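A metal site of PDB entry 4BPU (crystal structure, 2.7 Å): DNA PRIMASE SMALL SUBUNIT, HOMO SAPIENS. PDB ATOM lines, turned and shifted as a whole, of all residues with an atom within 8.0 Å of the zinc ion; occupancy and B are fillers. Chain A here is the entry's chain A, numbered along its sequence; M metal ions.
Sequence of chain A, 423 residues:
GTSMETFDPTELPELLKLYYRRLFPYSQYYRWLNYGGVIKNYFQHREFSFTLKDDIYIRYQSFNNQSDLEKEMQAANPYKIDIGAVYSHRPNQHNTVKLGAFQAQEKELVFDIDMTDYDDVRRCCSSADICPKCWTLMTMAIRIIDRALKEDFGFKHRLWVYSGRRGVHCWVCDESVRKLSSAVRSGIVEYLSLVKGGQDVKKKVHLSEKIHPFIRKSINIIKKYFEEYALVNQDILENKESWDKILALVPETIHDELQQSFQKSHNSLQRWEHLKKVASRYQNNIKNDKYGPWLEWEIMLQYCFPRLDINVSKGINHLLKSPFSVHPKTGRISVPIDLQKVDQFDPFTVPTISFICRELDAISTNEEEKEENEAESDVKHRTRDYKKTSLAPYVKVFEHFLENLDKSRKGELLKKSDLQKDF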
ATOM      1  N   MET A 115      -6.752  19.107 -15.029  1.00  0.00           N
ATOM      2  CA  MET A 115      -5.380  19.559 -14.899  1.00  0.00           C
ATOM      3  C   MET A 115      -4.589  19.330 -16.196  1.00  0.00           C
ATOM      4  O   MET A 115      -3.689  20.091 -16.542  1.00  0.00           O
ATOM      5  CB  MET A 115      -4.701  18.854 -13.740  1.00  0.00           C
ATOM      6  CG  MET A 115      -3.445  19.562 -13.250  1.00  0.00           C
ATOM      7  SD  MET A 115      -3.828  21.142 -12.464  1.00  0.00           S
ATOM      8  CE  MET A 115      -4.479  20.565 -10.932  1.00  0.00           C
ATOM      9  N   ARG A 122       2.377  24.224 -17.038  1.00  0.00           N
ATOM     10  CA  ARG A 122       2.877  23.722 -15.758  1.00  0.00           C
ATOM     11  C   ARG A 122       4.102  22.856 -16.023  1.00  0.00           C
ATOM     12  O   ARG A 122       4.158  22.161 -17.045  1.00  0.00           O
ATOM     13  CB  ARG A 122       1.816  22.947 -14.980  1.00  0.00           C
ATOM     14  CG  ARG A 122       1.211  21.773 -15.726  1.00  0.00           C
ATOM     15  CD  ARG A 122       0.506  20.857 -14.779  1.00  0.00           C
ATOM     16  NE  ARG A 122      -0.117  19.730 -15.473  1.00  0.00           N
ATOM     17  CZ  ARG A 122      -0.578  18.637 -14.867  1.00  0.00           C
ATOM     18  NH1 ARG A 122      -0.476  18.496 -13.554  1.00  0.00           N
ATOM     19  NH2 ARG A 122      -1.138  17.670 -15.596  1.00  0.00           N
ATOM     20  N   ARG A 123       5.035  22.875 -15.080  1.00  0.00           N
ATOM     21  CA  ARG A 123       6.343  22.244 -15.292  1.00  0.00           C
ATOM     22  C   ARG A 123       6.598  21.048 -14.382  1.00  0.00           C
ATOM     23  O   ARG A 123       7.497  20.252 -14.653  1.00  0.00           O
ATOM     24  CB  ARG A 123       7.423  23.293 -15.047  1.00  0.00           C
ATOM     25  CG  ARG A 123       7.357  24.495 -15.978  1.00  0.00           C
ATOM     26  CD  ARG A 123       8.453  25.506 -15.636  1.00  0.00           C
ATOM     27  NE  ARG A 123       9.787  25.029 -16.002  1.00  0.00           N
ATOM     28  CZ  ARG A 123      10.889  25.199 -15.262  1.00  0.00           C
ATOM     29  NH1 ARG A 123      10.826  25.812 -14.103  1.00  0.00           N
ATOM     30  NH2 ARG A 123      12.054  24.737 -15.694  1.00  0.00           N
ATOM     31  N   CYS A 124       5.791  20.890 -13.345  1.00  0.00           N
ATOM     32  CA  CYS A 124       6.019  19.850 -12.352  1.00  0.00           C
ATOM     33  C   CYS A 124       5.494  18.498 -12.825  1.00  0.00           C
ATOM     34  O   CYS A 124       6.136  17.476 -12.593  1.00  0.00           O
ATOM     35  CB  CYS A 124       5.351  20.241 -11.039  1.00  0.00           C
ATOM     36  SG  CYS A 124       3.670  20.795 -11.280  1.00  0.00           S
ATOM     37  N   CYS A 125       4.351  18.498 -13.497  1.00  0.00           N
ATOM     38  CA  CYS A 125       3.702  17.249 -13.915  1.00  0.00           C
ATOM     39  C   CYS A 125       3.240  17.329 -15.346  1.00  0.00           C
ATOM     40  O   CYS A 125       3.296  18.383 -15.976  1.00  0.00           O
ATOM     41  CB  CYS A 125       2.481  16.943 -13.045  1.00  0.00           C
ATOM     42  SG  CYS A 125       2.740  16.972 -11.278  1.00  0.00           S
ATOM     43  N   SER A 126       2.687  16.222 -15.844  1.00  0.00           N
ATOM     44  CA  SER A 126       2.087  16.194 -17.174  1.00  0.00           C
ATOM     45  C   SER A 126       0.980  15.167 -17.150  1.00  0.00           C
ATOM     46  O   SER A 126       0.944  14.305 -16.259  1.00  0.00           O
ATOM     47  CB  SER A 126       3.107  15.871 -18.276  1.00  0.00           C
ATOM     48  OG  SER A 126       3.775  14.632 -18.059  1.00  0.00           O
ATOM     49  N   ASP A 129      -0.844  13.261 -13.952  1.00  0.00           N
ATOM     50  CA  ASP A 129      -0.115  13.469 -12.718  1.00  0.00           C
ATOM     51  C   ASP A 129      -0.522  14.794 -12.116  1.00  0.00           C
ATOM     52  O   ASP A 129      -0.696  15.775 -12.842  1.00  0.00           O
ATOM     53  CB  ASP A 129       1.410  13.450 -12.927  1.00  0.00           C
ATOM     54  CG  ASP A 129       2.003  12.077 -12.760  1.00  0.00           C
ATOM     55  OD1 ASP A 129       1.465  11.292 -11.956  1.00  0.00           O
ATOM     56  OD2 ASP A 129       3.009  11.784 -13.461  1.00  0.00           O
ATOM     57  N   ILE A 130      -0.709  14.817 -10.798  1.00  0.00           N
ATOM     58  CA  ILE A 130      -0.935  16.057 -10.081  1.00  0.00           C
ATOM     59  C   ILE A 130      -0.033  16.106  -8.849  1.00  0.00           C
ATOM     60  O   ILE A 130       0.416  15.070  -8.354  1.00  0.00           O
ATOM     61  CB  ILE A 130      -2.400  16.218  -9.666  1.00  0.00           C
ATOM     62  CG1 ILE A 130      -2.845  15.081  -8.731  1.00  0.00           C
ATOM     63  CG2 ILE A 130      -3.287  16.248 -10.895  1.00  0.00           C
ATOM     64  CD1 ILE A 130      -4.061  15.455  -7.890  1.00  0.00           C
ATOM     65  N   CYS A 131       0.244  17.322  -8.389  1.00  0.00           N
ATOM     66  CA  CYS A 131       1.109  17.543  -7.236  1.00  0.00           C
ATOM     67  C   CYS A 131       0.655  18.816  -6.518  1.00  0.00           C
ATOM     68  O   CYS A 131      -0.118  19.591  -7.065  1.00  0.00           O
ATOM     69  CB  CYS A 131       2.587  17.647  -7.660  1.00  0.00           C
ATOM     70  SG  CYS A 131       3.020  19.246  -8.400  1.00  0.00           S
ATOM     71  N   PRO A 132       1.147  19.041  -5.298  1.00  0.00           N
ATOM     72  CA  PRO A 132       0.761  20.250  -4.565  1.00  0.00           C
ATOM     73  C   PRO A 132       1.195  21.545  -5.264  1.00  0.00           C
ATOM     74  O   PRO A 132       0.566  22.582  -5.087  1.00  0.00           O
ATOM     75  CB  PRO A 132       1.498  20.081  -3.221  1.00  0.00           C
ATOM     76  CG  PRO A 132       1.683  18.608  -3.075  1.00  0.00           C
ATOM     77  CD  PRO A 132       1.931  18.108  -4.478  1.00  0.00           C
ATOM     78  N   LYS A 133       2.206  21.460  -6.120  1.00  0.00           N
ATOM     79  CA  LYS A 133       2.715  22.647  -6.785  1.00  0.00           C
ATOM     80  C   LYS A 133       1.829  23.116  -7.945  1.00  0.00           C
ATOM     81  O   LYS A 133       1.838  24.294  -8.280  1.00  0.00           O
ATOM     82  CB  LYS A 133       4.133  22.392  -7.279  1.00  0.00           C
ATOM     83  CG  LYS A 133       5.118  22.126  -6.138  1.00  0.00           C
ATOM     84  CD  LYS A 133       6.563  22.398  -6.555  1.00  0.00           C
ATOM     85  CE  LYS A 133       7.121  21.288  -7.432  1.00  0.00           C
ATOM     86  NZ  LYS A 133       8.396  21.698  -8.103  1.00  0.00           N
ATOM     87  N   CYS A 134       1.071  22.199  -8.554  1.00  0.00           N
ATOM     88  CA  CYS A 134       0.185  22.570  -9.672  1.00  0.00           C
ATOM     89  C   CYS A 134      -1.296  22.642  -9.262  1.00  0.00           C
ATOM     90  O   CYS A 134      -2.096  23.232  -9.976  1.00  0.00           O
ATOM     91  CB  CYS A 134       0.344  21.612 -10.879  1.00  0.00           C
ATOM     92  SG  CYS A 134       0.398  19.827 -10.515  1.00  0.00           S
ATOM     93  N   TRP A 135      -1.655  22.053  -8.121  1.00  0.00           N
ATOM     94  CA  TRP A 135      -3.059  22.004  -7.729  1.00  0.00           C
ATOM     95  C   TRP A 135      -3.639  23.397  -7.518  1.00  0.00           C
ATOM     96  O   TRP A 135      -4.850  23.616  -7.701  1.00  0.00           O
ATOM     97  CB  TRP A 135      -3.229  21.182  -6.455  1.00  0.00           C
ATOM     98  CG  TRP A 135      -4.671  21.024  -6.109  1.00  0.00           C
ATOM     99  CD1 TRP A 135      -5.351  21.652  -5.114  1.00  0.00           C
ATOM    100  CD2 TRP A 135      -5.624  20.198  -6.786  1.00  0.00           C
ATOM    101  NE1 TRP A 135      -6.664  21.264  -5.121  1.00  0.00           N
ATOM    102  CE2 TRP A 135      -6.860  20.371  -6.144  1.00  0.00           C
ATOM    103  CE3 TRP A 135      -5.550  19.327  -7.874  1.00  0.00           C
ATOM    104  CZ2 TRP A 135      -8.006  19.705  -6.549  1.00  0.00           C
ATOM    105  CZ3 TRP A 135      -6.686  18.658  -8.277  1.00  0.00           C
ATOM    106  CH2 TRP A 135      -7.902  18.856  -7.615  1.00  0.00           C
ATOM    107  N   LEU A 137      -3.709  25.651  -9.397  1.00  0.00           N
ATOM    108  CA  LEU A 137      -4.435  25.972 -10.614  1.00  0.00           C
ATOM    109  C   LEU A 137      -5.920  25.695 -10.445  1.00  0.00           C
ATOM    110  O   LEU A 137      -6.755  26.473 -10.896  1.00  0.00           O
ATOM    111  CB  LEU A 137      -3.872  25.198 -11.803  1.00  0.00           C
ATOM    112  CG  LEU A 137      -2.526  25.670 -12.359  1.00  0.00           C
ATOM    113  CD1 LEU A 137      -2.033  24.653 -13.375  1.00  0.00           C
ATOM    114  CD2 LEU A 137      -2.611  27.074 -12.998  1.00  0.00           C
ATOM    115  N   TYR A 229       2.675  30.551  -6.902  1.00  0.00           N
ATOM    116  CA  TYR A 229       2.437  29.443  -7.824  1.00  0.00           C
ATOM    117  C   TYR A 229       3.403  29.435  -8.995  1.00  0.00           C
ATOM    118  O   TYR A 229       4.019  28.409  -9.292  1.00  0.00           O
ATOM    119  CB  TYR A 229       0.993  29.468  -8.372  1.00  0.00           C
ATOM    120  CG  TYR A 229       0.893  28.629  -9.632  1.00  0.00           C
ATOM    121  CD1 TYR A 229       0.884  27.238  -9.564  1.00  0.00           C
ATOM    122  CD2 TYR A 229       0.858  29.221 -10.874  1.00  0.00           C
ATOM    123  CE1 TYR A 229       0.838  26.466 -10.714  1.00  0.00           C
ATOM    124  CE2 TYR A 229       0.804  28.460 -12.025  1.00  0.00           C
ATOM    125  CZ  TYR A 229       0.785  27.089 -11.948  1.00  0.00           C
ATOM    126  OH  TYR A 229       0.732  26.339 -13.098  1.00  0.00           O
ATOM    127  N   GLN A 234       6.481  26.871  -9.574  1.00  0.00           N
ATOM    128  CA  GLN A 234       6.596  26.472 -10.969  1.00  0.00           C
ATOM    129  C   GLN A 234       7.882  27.015 -11.590  1.00  0.00           C
ATOM    130  O   GLN A 234       8.474  26.378 -12.447  1.00  0.00           O
ATOM    131  CB  GLN A 234       5.401  26.943 -11.787  1.00  0.00           C
ATOM    132  CG  GLN A 234       4.155  26.125 -11.532  1.00  0.00           C
ATOM    133  CD  GLN A 234       4.259  24.707 -12.044  1.00  0.00           C
ATOM    134  OE1 GLN A 234       4.765  24.471 -13.152  1.00  0.00           O
ATOM    135  NE2 GLN A 234       3.780  23.753 -11.260  1.00  0.00           N
ATOM    136  N   PHE A 348      -5.019  14.875  -1.868  1.00  0.00           N
ATOM    137  CA  PHE A 348      -4.179  13.762  -1.441  1.00  0.00           C
ATOM    138  C   PHE A 348      -4.553  13.218  -0.057  1.00  0.00           C
ATOM    139  O   PHE A 348      -4.026  12.193   0.370  1.00  0.00           O
ATOM    140  CB  PHE A 348      -2.723  14.193  -1.455  1.00  0.00           C
ATOM    141  CG  PHE A 348      -2.258  14.656  -2.808  1.00  0.00           C
ATOM    142  CD1 PHE A 348      -1.886  13.753  -3.778  1.00  0.00           C
ATOM    143  CD2 PHE A 348      -2.214  16.008  -3.112  1.00  0.00           C
ATOM    144  CE1 PHE A 348      -1.477  14.165  -5.017  1.00  0.00           C
ATOM    145  CE2 PHE A 348      -1.799  16.442  -4.357  1.00  0.00           C
ATOM    146  CZ  PHE A 348      -1.436  15.516  -5.312  1.00  0.00           C
HETATM  147 ZN    ZN M   1       2.503  19.052 -10.367  1.00  0.00          ZN
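SG of Cys 131 sits close to N of Lys 133. The side-chain sulfur (SG) of Cys 134 lies close to the guanidinium group (NH1) of Arg 122 (3.4 Å). The side-chain amide nitrogen (NE2) of Gln 234 lies close to the side-chain sulfur (SG) of Cys 124, at 3.0 Å.
Of the 17 residues printed, 4 come within 4 Å of the zinc ion.
The zinc ion is bound by the side-chain sulfur (SG) of Cys 131, the side-chain sulfur (SG) of Cys 134, the side-chain sulfur (SG) of Cys 125 and the side-chain sulfur (SG) of Cys 124. The zinc ion has four donor atoms within binding distance.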
